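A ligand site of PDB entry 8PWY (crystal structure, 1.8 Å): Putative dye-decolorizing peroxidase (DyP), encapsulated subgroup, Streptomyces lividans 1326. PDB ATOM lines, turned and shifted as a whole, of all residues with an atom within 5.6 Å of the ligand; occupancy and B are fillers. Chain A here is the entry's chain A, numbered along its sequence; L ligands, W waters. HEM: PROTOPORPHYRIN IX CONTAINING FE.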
ATOM      1  N   ASP A 140     -16.228  25.377   4.998  1.00  0.00           N
ATOM      2  CA  ASP A 140     -15.407  26.176   4.099  1.00  0.00           C
ATOM      3  C   ASP A 140     -16.201  27.425   3.757  1.00  0.00           C
ATOM      4  O   ASP A 140     -17.264  27.695   4.256  1.00  0.00           O
ATOM      5  CB  ASP A 140     -14.941  25.328   2.898  1.00  0.00           C
ATOM      6  CG  ASP A 140     -16.047  24.771   2.027  1.00  0.00           C
ATOM      7  OD1 ASP A 140     -17.123  25.417   1.990  1.00  0.00           O
ATOM      8  OD2 ASP A 140     -15.813  23.674   1.438  1.00  0.00           O
ATOM      9  N   LEU A 142     -17.686  28.235   1.115  1.00  0.00           N
ATOM     10  CA  LEU A 142     -18.971  28.017   0.457  1.00  0.00           C
ATOM     11  C   LEU A 142     -20.041  27.618   1.452  1.00  0.00           C
ATOM     12  O   LEU A 142     -21.170  27.455   1.065  1.00  0.00           O
ATOM     13  CB  LEU A 142     -18.814  26.937  -0.614  1.00  0.00           C
ATOM     14  CG  LEU A 142     -17.744  27.212  -1.690  1.00  0.00           C
ATOM     15  CD1 LEU A 142     -17.626  26.048  -2.657  1.00  0.00           C
ATOM     16  CD2 LEU A 142     -18.039  28.510  -2.422  1.00  0.00           C
ATOM     17  N   PHE A 144     -20.172  24.771   3.313  1.00  0.00           N
ATOM     18  CA  PHE A 144     -20.328  23.325   3.430  1.00  0.00           C
ATOM     19  C   PHE A 144     -19.236  22.771   4.345  1.00  0.00           C
ATOM     20  O   PHE A 144     -18.117  23.288   4.361  1.00  0.00           O
ATOM     21  CB  PHE A 144     -20.295  22.647   2.068  1.00  0.00           C
ATOM     22  CG  PHE A 144     -21.584  22.750   1.291  1.00  0.00           C
ATOM     23  CD1 PHE A 144     -21.984  23.943   0.734  1.00  0.00           C
ATOM     24  CD2 PHE A 144     -22.386  21.656   1.097  1.00  0.00           C
ATOM     25  CE1 PHE A 144     -23.180  24.038   0.025  1.00  0.00           C
ATOM     26  CE2 PHE A 144     -23.579  21.753   0.397  1.00  0.00           C
ATOM     27  CZ  PHE A 144     -23.973  22.942  -0.118  1.00  0.00           C
ATOM     28  N   VAL A 145     -19.561  21.689   5.064  1.00  0.00           N
ATOM     29  CA  VAL A 145     -18.573  20.966   5.855  1.00  0.00           C
ATOM     30  C   VAL A 145     -17.545  20.370   4.878  1.00  0.00           C
ATOM     31  O   VAL A 145     -17.910  19.824   3.856  1.00  0.00           O
ATOM     32  CB  VAL A 145     -19.214  19.873   6.745  1.00  0.00           C
ATOM     33  CG1 VAL A 145     -18.191  19.131   7.560  1.00  0.00           C
ATOM     34  CG2 VAL A 145     -20.307  20.411   7.659  1.00  0.00           C
ATOM     35  N   ASP A 146     -16.270  20.448   5.246  1.00  0.00           N
ATOM     36  CA  ASP A 146     -15.148  20.153   4.368  1.00  0.00           C
ATOM     37  C   ASP A 146     -14.204  19.237   5.149  1.00  0.00           C
ATOM     38  O   ASP A 146     -13.699  19.626   6.179  1.00  0.00           O
ATOM     39  CB  ASP A 146     -14.533  21.508   3.925  1.00  0.00           C
ATOM     40  CG  ASP A 146     -13.513  21.447   2.785  1.00  0.00           C
ATOM     41  OD1 ASP A 146     -12.679  20.527   2.874  1.00  0.00           O
ATOM     42  OD2 ASP A 146     -13.552  22.375   1.821  1.00  0.00           O
ATOM     43  N   GLY A 147     -14.015  17.994   4.691  1.00  0.00           N
ATOM     44  CA  GLY A 147     -13.208  17.023   5.422  1.00  0.00           C
ATOM     45  C   GLY A 147     -13.899  15.665   5.664  1.00  0.00           C
ATOM     46  O   GLY A 147     -13.238  14.700   5.991  1.00  0.00           O
ATOM     47  N   THR A 148     -15.225  15.605   5.492  1.00  0.00           N
ATOM     48  CA  THR A 148     -16.052  14.544   6.029  1.00  0.00           C
ATOM     49  C   THR A 148     -15.607  13.163   5.548  1.00  0.00           C
ATOM     50  O   THR A 148     -15.490  12.228   6.338  1.00  0.00           O
ATOM     51  CB  THR A 148     -17.498  14.755   5.604  1.00  0.00           C
ATOM     52  OG1 THR A 148     -17.803  16.101   5.971  1.00  0.00           O
ATOM     53  CG2 THR A 148     -18.435  13.795   6.296  1.00  0.00           C
ATOM     54  N   GLU A 149     -15.343  13.032   4.254  1.00  0.00           N
ATOM     55  CA  GLU A 149     -15.026  11.742   3.698  1.00  0.00           C
ATOM     56  C   GLU A 149     -13.536  11.477   3.627  1.00  0.00           C
ATOM     57  O   GLU A 149     -13.118  10.505   3.026  1.00  0.00           O
ATOM     58  CB  GLU A 149     -15.710  11.568   2.340  1.00  0.00           C
ATOM     59  CG  GLU A 149     -17.211  11.252   2.493  1.00  0.00           C
ATOM     60  CD  GLU A 149     -17.548   9.997   3.295  1.00  0.00           C
ATOM     61  OE1 GLU A 149     -17.079   8.973   2.936  1.00  0.00           O
ATOM     62  OE2 GLU A 149     -18.206  10.076   4.301  1.00  0.00           O
ATOM     63  N   ASN A 150     -12.723  12.251   4.303  1.00  0.00           N
ATOM     64  CA  ASN A 150     -11.311  11.906   4.381  1.00  0.00           C
ATOM     65  C   ASN A 150     -11.154  10.533   4.992  1.00  0.00           C
ATOM     66  O   ASN A 150     -11.866  10.223   5.946  1.00  0.00           O
ATOM     67  CB  ASN A 150     -10.482  12.853   5.241  1.00  0.00           C
ATOM     68  CG  ASN A 150      -9.909  14.002   4.469  1.00  0.00           C
ATOM     69  OD1 ASN A 150      -9.525  13.846   3.301  1.00  0.00           O
ATOM     70  ND2 ASN A 150      -9.840  15.159   5.085  1.00  0.00           N
ATOM     71  N   GLN A 178      -3.359  23.861  -4.505  1.00  0.00           N
ATOM     72  CA  GLN A 178      -3.966  24.856  -5.360  1.00  0.00           C
ATOM     73  C   GLN A 178      -4.654  25.897  -4.470  1.00  0.00           C
ATOM     74  O   GLN A 178      -5.470  25.554  -3.635  1.00  0.00           O
ATOM     75  CB  GLN A 178      -5.032  24.235  -6.253  1.00  0.00           C
ATOM     76  CG  GLN A 178      -4.544  23.245  -7.291  1.00  0.00           C
ATOM     77  CD  GLN A 178      -5.731  22.729  -8.059  1.00  0.00           C
ATOM     78  OE1 GLN A 178      -6.604  22.055  -7.501  1.00  0.00           O
ATOM     79  NE2 GLN A 178      -5.822  23.147  -9.318  1.00  0.00           N
ATOM     80  N   TYR A 180      -7.497  28.516  -4.367  1.00  0.00           N
ATOM     81  CA  TYR A 180      -8.723  28.853  -5.085  1.00  0.00           C
ATOM     82  C   TYR A 180      -9.337  30.125  -4.482  1.00  0.00           C
ATOM     83  O   TYR A 180      -9.413  30.271  -3.264  1.00  0.00           O
ATOM     84  CB  TYR A 180      -9.772  27.756  -4.950  1.00  0.00           C
ATOM     85  CG  TYR A 180      -9.571  26.532  -5.824  1.00  0.00           C
ATOM     86  CD1 TYR A 180     -10.048  26.469  -7.113  1.00  0.00           C
ATOM     87  CD2 TYR A 180      -8.831  25.459  -5.362  1.00  0.00           C
ATOM     88  CE1 TYR A 180      -9.853  25.346  -7.910  1.00  0.00           C
ATOM     89  CE2 TYR A 180      -8.575  24.354  -6.160  1.00  0.00           C
ATOM     90  CZ  TYR A 180      -9.128  24.271  -7.431  1.00  0.00           C
ATOM     91  OH  TYR A 180      -8.909  23.129  -8.178  1.00  0.00           O
ATOM     92  N   HIS A 182     -13.056  32.212  -4.603  1.00  0.00           N
ATOM     93  CA  HIS A 182     -14.441  31.943  -4.894  1.00  0.00           C
ATOM     94  C   HIS A 182     -15.134  33.225  -5.298  1.00  0.00           C
ATOM     95  O   HIS A 182     -14.809  34.289  -4.790  1.00  0.00           O
ATOM     96  CB  HIS A 182     -15.142  31.331  -3.676  1.00  0.00           C
ATOM     97  CG  HIS A 182     -14.571  30.025  -3.260  1.00  0.00           C
ATOM     98  ND1 HIS A 182     -14.702  28.903  -4.046  1.00  0.00           N
ATOM     99  CD2 HIS A 182     -13.912  29.661  -2.146  1.00  0.00           C
ATOM    100  CE1 HIS A 182     -14.095  27.895  -3.402  1.00  0.00           C
ATOM    101  NE2 HIS A 182     -13.622  28.310  -2.238  1.00  0.00           N
ATOM    102  N   ILE A 199     -22.394  20.519  -4.900  1.00  0.00           N
ATOM    103  CA  ILE A 199     -21.463  19.807  -4.050  1.00  0.00           C
ATOM    104  C   ILE A 199     -21.742  18.299  -4.062  1.00  0.00           C
ATOM    105  O   ILE A 199     -20.814  17.519  -4.184  1.00  0.00           O
ATOM    106  CB  ILE A 199     -21.532  20.377  -2.621  1.00  0.00           C
ATOM    107  CG1 ILE A 199     -21.173  21.858  -2.587  1.00  0.00           C
ATOM    108  CG2 ILE A 199     -20.661  19.586  -1.660  1.00  0.00           C
ATOM    109  CD1 ILE A 199     -19.787  22.175  -2.982  1.00  0.00           C
ATOM    110  N   ARG A 201     -23.827  17.026  -1.402  1.00  0.00           N
ATOM    111  CA  ARG A 201     -24.210  16.699  -0.058  1.00  0.00           C
ATOM    112  C   ARG A 201     -25.194  17.745   0.435  1.00  0.00           C
ATOM    113  O   ARG A 201     -25.269  18.801  -0.136  1.00  0.00           O
ATOM    114  CB  ARG A 201     -22.990  16.700   0.892  1.00  0.00           C
ATOM    115  CG  ARG A 201     -21.830  15.842   0.408  1.00  0.00           C
ATOM    116  CD  ARG A 201     -20.651  15.787   1.330  1.00  0.00           C
ATOM    117  NE  ARG A 201     -20.926  15.092   2.575  1.00  0.00           N
ATOM    118  CZ  ARG A 201     -20.834  13.778   2.765  1.00  0.00           C
ATOM    119  NH1 ARG A 201     -20.260  12.987   1.882  1.00  0.00           N
ATOM    120  NH2 ARG A 201     -21.296  13.223   3.870  1.00  0.00           N
ATOM    121  N   ASP A 206     -24.919  17.741   6.217  1.00  0.00           N
ATOM    122  CA  ASP A 206     -23.754  17.085   5.647  1.00  0.00           C
ATOM    123  C   ASP A 206     -24.019  15.608   5.313  1.00  0.00           C
ATOM    124  O   ASP A 206     -23.101  14.801   5.264  1.00  0.00           O
ATOM    125  CB  ASP A 206     -22.529  17.166   6.547  1.00  0.00           C
ATOM    126  CG  ASP A 206     -21.209  16.916   5.841  1.00  0.00           C
ATOM    127  OD1 ASP A 206     -21.123  17.039   4.563  1.00  0.00           O
ATOM    128  OD2 ASP A 206     -20.250  16.615   6.543  1.00  0.00           O
ATOM    129  N   GLU A 208     -24.769  12.826   2.545  1.00  0.00           N
ATOM    130  CA  GLU A 208     -24.576  12.680   1.116  1.00  0.00           C
ATOM    131  C   GLU A 208     -25.925  12.541   0.398  1.00  0.00           C
ATOM    132  O   GLU A 208     -26.835  11.945   0.909  1.00  0.00           O
ATOM    133  CB  GLU A 208     -23.680  11.466   0.944  1.00  0.00           C
ATOM    134  CG  GLU A 208     -23.280  11.232  -0.492  1.00  0.00           C
ATOM    135  CD  GLU A 208     -22.109  10.268  -0.645  1.00  0.00           C
ATOM    136  OE1 GLU A 208     -21.451   9.901   0.352  1.00  0.00           O
ATOM    137  OE2 GLU A 208     -21.825   9.974  -1.761  1.00  0.00           O
ATOM    138  N   HIS A 219     -19.456  17.795  -7.298  1.00  0.00           N
ATOM    139  CA  HIS A 219     -18.074  17.701  -6.876  1.00  0.00           C
ATOM    140  C   HIS A 219     -17.776  16.312  -6.309  1.00  0.00           C
ATOM    141  O   HIS A 219     -16.744  15.697  -6.629  1.00  0.00           O
ATOM    142  CB  HIS A 219     -17.771  18.813  -5.877  1.00  0.00           C
ATOM    143  CG  HIS A 219     -16.390  18.790  -5.383  1.00  0.00           C
ATOM    144  ND1 HIS A 219     -15.305  18.897  -6.215  1.00  0.00           N
ATOM    145  CD2 HIS A 219     -15.913  18.725  -4.121  1.00  0.00           C
ATOM    146  CE1 HIS A 219     -14.195  18.885  -5.473  1.00  0.00           C
ATOM    147  NE2 HIS A 219     -14.543  18.783  -4.177  1.00  0.00           N
ATOM    148  N   VAL A 220     -18.719  15.812  -5.507  1.00  0.00           N
ATOM    149  CA  VAL A 220     -18.545  14.519  -4.887  1.00  0.00           C
ATOM    150  C   VAL A 220     -18.573  13.407  -5.945  1.00  0.00           C
ATOM    151  O   VAL A 220     -17.870  12.422  -5.810  1.00  0.00           O
ATOM    152  CB  VAL A 220     -19.584  14.287  -3.787  1.00  0.00           C
ATOM    153  CG1 VAL A 220     -19.725  12.817  -3.445  1.00  0.00           C
ATOM    154  CG2 VAL A 220     -19.215  15.098  -2.554  1.00  0.00           C
ATOM    155  N   THR A 223     -15.136  13.478  -7.889  1.00  0.00           N
ATOM    156  CA  THR A 223     -13.930  13.161  -7.125  1.00  0.00           C
ATOM    157  C   THR A 223     -14.035  11.792  -6.451  1.00  0.00           C
ATOM    158  O   THR A 223     -13.150  11.445  -5.683  1.00  0.00           O
ATOM    159  CB  THR A 223     -13.624  14.267  -6.094  1.00  0.00           C
ATOM    160  OG1 THR A 223     -14.705  14.423  -5.168  1.00  0.00           O
ATOM    161  CG2 THR A 223     -13.294  15.585  -6.789  1.00  0.00           C
ATOM    162  N   SER A 224     -15.080  11.013  -6.759  1.00  0.00           N
ATOM    163  CA  SER A 224     -15.159   9.607  -6.386  1.00  0.00           C
ATOM    164  C   SER A 224     -14.597   8.742  -7.519  1.00  0.00           C
ATOM    165  O   SER A 224     -15.097   8.805  -8.644  1.00  0.00           O
ATOM    166  CB  SER A 224     -16.569   9.175  -6.099  1.00  0.00           C
ATOM    167  OG  SER A 224     -17.072   9.886  -4.997  1.00  0.00           O
ATOM    168  N   ILE A 235      -7.611  10.186  -1.237  1.00  0.00           N
ATOM    169  CA  ILE A 235      -6.574  11.130  -0.842  1.00  0.00           C
ATOM    170  C   ILE A 235      -6.926  11.714   0.516  1.00  0.00           C
ATOM    171  O   ILE A 235      -8.033  11.580   0.984  1.00  0.00           O
ATOM    172  CB  ILE A 235      -6.370  12.246  -1.883  1.00  0.00           C
ATOM    173  CG1 ILE A 235      -7.541  13.208  -1.933  1.00  0.00           C
ATOM    174  CG2 ILE A 235      -6.084  11.671  -3.264  1.00  0.00           C
ATOM    175  CD1 ILE A 235      -7.253  14.408  -2.815  1.00  0.00           C
ATOM    176  N   ARG A 237      -7.099  15.285   2.447  1.00  0.00           N
ATOM    177  CA  ARG A 237      -7.188  16.704   2.245  1.00  0.00           C
ATOM    178  C   ARG A 237      -7.181  17.431   3.573  1.00  0.00           C
ATOM    179  O   ARG A 237      -7.660  16.911   4.569  1.00  0.00           O
ATOM    180  CB  ARG A 237      -8.489  17.048   1.508  1.00  0.00           C
ATOM    181  CG  ARG A 237      -8.587  16.455   0.118  1.00  0.00           C
ATOM    182  CD  ARG A 237      -9.981  16.561  -0.442  1.00  0.00           C
ATOM    183  NE  ARG A 237     -10.884  15.628   0.211  1.00  0.00           N
ATOM    184  CZ  ARG A 237     -11.939  15.980   0.958  1.00  0.00           C
ATOM    185  NH1 ARG A 237     -12.361  17.241   0.963  1.00  0.00           N
ATOM    186  NH2 ARG A 237     -12.594  15.062   1.667  1.00  0.00           N
ATOM    187  N   ASN A 239      -8.061  21.149   3.517  1.00  0.00           N
ATOM    188  CA  ASN A 239      -8.385  22.446   2.935  1.00  0.00           C
ATOM    189  C   ASN A 239      -8.630  23.494   4.042  1.00  0.00           C
ATOM    190  O   ASN A 239      -9.232  23.225   5.081  1.00  0.00           O
ATOM    191  CB  ASN A 239      -9.652  22.359   2.094  1.00  0.00           C
ATOM    192  CG  ASN A 239      -9.566  21.365   0.952  1.00  0.00           C
ATOM    193  OD1 ASN A 239      -8.493  20.892   0.578  1.00  0.00           O
ATOM    194  ND2 ASN A 239     -10.718  21.029   0.393  1.00  0.00           N
ATOM    195  N   THR A 252     -10.349  29.126  -0.676  1.00  0.00           N
ATOM    196  CA  THR A 252     -10.046  27.808  -0.136  1.00  0.00           C
ATOM    197  C   THR A 252      -8.641  27.457  -0.570  1.00  0.00           C
ATOM    198  O   THR A 252      -8.346  27.482  -1.767  1.00  0.00           O
ATOM    199  CB  THR A 252     -11.058  26.768  -0.616  1.00  0.00           C
ATOM    200  OG1 THR A 252     -12.398  27.083  -0.207  1.00  0.00           O
ATOM    201  CG2 THR A 252     -10.667  25.369  -0.185  1.00  0.00           C
ATOM    202  N   PHE A 254      -6.439  24.516  -1.123  1.00  0.00           N
ATOM    203  CA  PHE A 254      -6.538  23.076  -1.284  1.00  0.00           C
ATOM    204  C   PHE A 254      -5.160  22.450  -1.104  1.00  0.00           C
ATOM    205  O   PHE A 254      -4.200  22.879  -1.736  1.00  0.00           O
ATOM    206  CB  PHE A 254      -7.044  22.698  -2.681  1.00  0.00           C
ATOM    207  CG  PHE A 254      -6.953  21.237  -2.964  1.00  0.00           C
ATOM    208  CD1 PHE A 254      -7.893  20.378  -2.475  1.00  0.00           C
ATOM    209  CD2 PHE A 254      -5.905  20.720  -3.664  1.00  0.00           C
ATOM    210  CE1 PHE A 254      -7.813  19.012  -2.721  1.00  0.00           C
ATOM    211  CE2 PHE A 254      -5.803  19.352  -3.885  1.00  0.00           C
ATOM    212  CZ  PHE A 254      -6.767  18.505  -3.422  1.00  0.00           C
ATOM    213  N   THR A 264      -4.407  11.877  -7.371  1.00  0.00           N
ATOM    214  CA  THR A 264      -4.804  13.267  -7.304  1.00  0.00           C
ATOM    215  C   THR A 264      -5.015  13.835  -8.695  1.00  0.00           C
ATOM    216  O   THR A 264      -5.977  14.585  -8.941  1.00  0.00           O
ATOM    217  CB  THR A 264      -3.776  14.084  -6.525  1.00  0.00           C
ATOM    218  OG1 THR A 264      -3.567  13.447  -5.270  1.00  0.00           O
ATOM    219  CG2 THR A 264      -4.276  15.456  -6.164  1.00  0.00           C
ATOM    220  N   MET A 267      -8.309  12.798 -10.311  1.00  0.00           N
ATOM    221  CA  MET A 267      -9.404  13.615  -9.798  1.00  0.00           C
ATOM    222  C   MET A 267      -9.401  14.985 -10.482  1.00  0.00           C
ATOM    223  O   MET A 267     -10.427  15.497 -10.905  1.00  0.00           O
ATOM    224  CB  MET A 267      -9.260  13.764  -8.288  1.00  0.00           C
ATOM    225  CG  MET A 267      -9.585  12.506  -7.542  1.00  0.00           C
ATOM    226  SD  MET A 267      -9.175  12.665  -5.789  1.00  0.00           S
ATOM    227  CE  MET A 267      -9.652  11.043  -5.187  1.00  0.00           C
ATOM    228  N   LEU A 268      -8.223  15.584 -10.631  1.00  0.00           N
ATOM    229  CA  LEU A 268      -8.140  16.889 -11.263  1.00  0.00           C
ATOM    230  C   LEU A 268      -8.601  16.864 -12.716  1.00  0.00           C
ATOM    231  O   LEU A 268      -9.251  17.807 -13.171  1.00  0.00           O
ATOM    232  CB  LEU A 268      -6.707  17.412 -11.169  1.00  0.00           C
ATOM    233  CG  LEU A 268      -6.290  17.989  -9.817  1.00  0.00           C
ATOM    234  CD1 LEU A 268      -4.805  18.289  -9.790  1.00  0.00           C
ATOM    235  CD2 LEU A 268      -7.039  19.257  -9.544  1.00  0.00           C
ATOM    236  N   MET A 271     -12.276  16.792 -12.862  1.00  0.00           N
ATOM    237  CA  MET A 271     -12.851  18.069 -12.499  1.00  0.00           C
ATOM    238  C   MET A 271     -12.737  19.062 -13.656  1.00  0.00           C
ATOM    239  O   MET A 271     -13.700  19.777 -13.927  1.00  0.00           O
ATOM    240  CB  MET A 271     -12.160  18.639 -11.268  1.00  0.00           C
ATOM    241  CG  MET A 271     -12.535  17.900  -9.970  1.00  0.00           C
ATOM    242  SD  MET A 271     -11.489  18.560  -8.585  1.00  0.00           S
ATOM    243  CE  MET A 271     -12.063  20.246  -8.500  1.00  0.00           C
ATOM    244  N   ILE A 283     -18.302  22.892  -9.129  1.00  0.00           N
ATOM    245  CA  ILE A 283     -17.683  23.740  -8.136  1.00  0.00           C
ATOM    246  C   ILE A 283     -16.757  24.773  -8.807  1.00  0.00           C
ATOM    247  O   ILE A 283     -16.525  25.854  -8.272  1.00  0.00           O
ATOM    248  CB  ILE A 283     -16.948  22.900  -7.076  1.00  0.00           C
ATOM    249  CG1 ILE A 283     -16.905  23.609  -5.724  1.00  0.00           C
ATOM    250  CG2 ILE A 283     -15.531  22.556  -7.472  1.00  0.00           C
ATOM    251  CD1 ILE A 283     -16.421  22.761  -4.548  1.00  0.00           C
ATOM    252  N   LEU A 284     -16.203  24.423 -10.001  1.00  0.00           N
ATOM    253  CA  LEU A 284     -15.295  25.311 -10.701  1.00  0.00           C
ATOM    254  C   LEU A 284     -16.036  26.500 -11.348  1.00  0.00           C
ATOM    255  O   LEU A 284     -15.406  27.485 -11.676  1.00  0.00           O
ATOM    256  CB  LEU A 284     -14.519  24.538 -11.762  1.00  0.00           C
ATOM    257  CG  LEU A 284     -13.610  23.450 -11.213  1.00  0.00           C
ATOM    258  CD1 LEU A 284     -12.963  22.722 -12.380  1.00  0.00           C
ATOM    259  CD2 LEU A 284     -12.536  24.031 -10.325  1.00  0.00           C
ATOM    260  N   SER A 287     -15.227  28.857  -8.500  1.00  0.00           N
ATOM    261  CA  SER A 287     -13.918  28.701  -7.880  1.00  0.00           C
ATOM    262  C   SER A 287     -12.870  28.798  -8.987  1.00  0.00           C
ATOM    263  O   SER A 287     -12.926  28.024  -9.955  1.00  0.00           O
ATOM    264  CB  SER A 287     -13.805  27.373  -7.125  1.00  0.00           C
ATOM    265  OG  SER A 287     -14.941  27.121  -6.322  1.00  0.00           O
HETATM  266  CHA HEM L   1     -15.087  16.374  -0.983  1.00  0.00           C
HETATM  267  CHB HEM L   1     -14.973  21.246  -0.996  1.00  0.00           C
HETATM  268  CHC HEM L   1     -11.363  21.149  -4.325  1.00  0.00           C
HETATM  269  CHD HEM L   1     -11.262  16.267  -3.844  1.00  0.00           C
HETATM  270  C1A HEM L   1     -15.364  17.724  -0.744  1.00  0.00           C
HETATM  271  C2A HEM L   1     -16.510  18.164  -0.006  1.00  0.00           C
HETATM  272  C3A HEM L   1     -16.456  19.531  -0.009  1.00  0.00           C
HETATM  273  C4A HEM L   1     -15.333  19.974  -0.751  1.00  0.00           C
HETATM  274  CMA HEM L   1     -17.447  20.404   0.727  1.00  0.00           C
HETATM  275  CAA HEM L   1     -17.560  17.285   0.674  1.00  0.00           C
HETATM  276  CBA HEM L   1     -17.187  16.929   2.138  1.00  0.00           C
HETATM  277  CGA HEM L   1     -15.921  16.143   2.206  1.00  0.00           C
HETATM  278  O1A HEM L   1     -14.879  16.816   2.409  1.00  0.00           O
HETATM  279  O2A HEM L   1     -15.958  14.869   2.055  1.00  0.00           O
HETATM  280  C1B HEM L   1     -13.982  21.626  -1.864  1.00  0.00           C
HETATM  281  C2B HEM L   1     -13.693  22.973  -2.186  1.00  0.00           C
HETATM  282  C3B HEM L   1     -12.662  22.993  -3.100  1.00  0.00           C
HETATM  283  C4B HEM L   1     -12.338  21.584  -3.428  1.00  0.00           C
HETATM  284  CMB HEM L   1     -14.273  24.236  -1.560  1.00  0.00           C
HETATM  285  CAB HEM L   1     -12.188  24.268  -3.705  1.00  0.00           C
HETATM  286  CBB HEM L   1     -12.124  24.350  -5.009  1.00  0.00           C
HETATM  287  C1C HEM L   1     -10.986  19.816  -4.493  1.00  0.00           C
HETATM  288  C2C HEM L   1      -9.938  19.300  -5.365  1.00  0.00           C
HETATM  289  C3C HEM L   1      -9.948  17.897  -5.241  1.00  0.00           C
HETATM  290  C4C HEM L   1     -10.989  17.574  -4.293  1.00  0.00           C
HETATM  291  CMC HEM L   1      -9.048  20.209  -6.213  1.00  0.00           C
HETATM  292  CAC HEM L   1      -9.131  16.805  -5.798  1.00  0.00           C
HETATM  293  CBC HEM L   1      -8.088  16.949  -6.569  1.00  0.00           C
HETATM  294  C1D HEM L   1     -12.274  15.930  -3.000  1.00  0.00           C
HETATM  295  C2D HEM L   1     -12.464  14.565  -2.631  1.00  0.00           C
HETATM  296  C3D HEM L   1     -13.579  14.567  -1.866  1.00  0.00           C
HETATM  297  C4D HEM L   1     -14.032  16.003  -1.802  1.00  0.00           C
HETATM  298  CMD HEM L   1     -11.644  13.340  -2.979  1.00  0.00           C
HETATM  299  CAD HEM L   1     -14.240  13.398  -1.136  1.00  0.00           C
HETATM  300  CBD HEM L   1     -15.270  12.756  -2.122  1.00  0.00           C
HETATM  301  CGD HEM L   1     -16.011  11.524  -1.556  1.00  0.00           C
HETATM  302  O1D HEM L   1     -15.572  10.394  -1.659  1.00  0.00           O
HETATM  303  O2D HEM L   1     -17.089  11.583  -0.944  1.00  0.00           O
HETATM  304  NA  HEM L   1     -14.700  18.869  -1.223  1.00  0.00           N
HETATM  305  NB  HEM L   1     -13.169  20.844  -2.634  1.00  0.00           N
HETATM  306  NC  HEM L   1     -11.548  18.751  -3.839  1.00  0.00           N
HETATM  307  ND  HEM L   1     -13.200  16.777  -2.485  1.00  0.00           N
HETATM  308 FE   HEM L   1     -13.206  18.745  -2.571  1.00  0.00          FE
HETATM  309  O   HOH W   1     -17.871  13.837   0.261  1.00  0.00           O
HETATM  310  O   HOH W   2     -12.967  10.406  -3.004  1.00  0.00           O
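Merely in contact with the ligand: Val 145, Gln 178, Asp 146, Thr 223, Phe 254, Asp 140, Tyr 180, Arg 201, Ile 283, Met 271, Thr 252, Ser 224, Met 267, Val 220, Leu 268, Phe 144, Asn 239, Thr 264 and Leu 142. Hydrophobic or aromatic side chains that line the ligand: Leu 142, Phe 144, Tyr 180, His 219, Val 220, Phe 254, Met 267, Leu 268, Met 271 and Ile 283. The nearest printed residue that does not touch the ligand is Ser 287 (4.1 Å).
FE of the ligand is bound by NE2 of His 219 (2.1 Å). The backbone NH (N) of Gly 147 sits at hydrogen-bond distance from an oxygen (O1A) of the ligand (2.7 Å). O2A of the ligand sits at hydrogen-bond distance from N of Glu 149 (2.9 Å). The guanidinium group (NH1) of Arg 237 lies within salt-bridge range of an oxygen (O1A) of the ligand, at 2.9 Å. The backbone NH of Thr 148 is in hydrogen-bond range of an oxygen (O1A) of the ligand (3.3 Å).
N of His 219 is in hydrogen-bond range of O of Ile 199 (3.4 Å). The guanidinium group of Arg 237 lies within salt-bridge range of the side-chain carboxylate of Asp 146. O of Gln 178 is in hydrogen-bond range of N of Phe 254. The side-chain amide oxygen of Gln 178 lies within hydrogen-bond range of the side-chain hydroxyl of Tyr 180, at 2.6 Å. N of Tyr 180 is in hydrogen-bond range of O of Thr 252 (2.9 Å). The guanidinium group (NH1) of Arg 201 is in salt-bridge range of the side-chain carboxylate (OE1) of Glu 208, at 3.6 Å. OG of Ser 224 is in hydrogen-bond range of O of Val 220 (2.8 Å). The backbone NH of Val 220 is in hydrogen-bond range of the backbone carbonyl oxygen of Ile 199 (3.0 Å).
Water W1 bridges an oxygen (O2D) of the ligand (2.7 Å) and the guanidinium group of Arg 201 (3.0 Å). Water W2 bridges O of Thr 223 (2.9 Å) and O1D of the ligand (2.9 Å).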
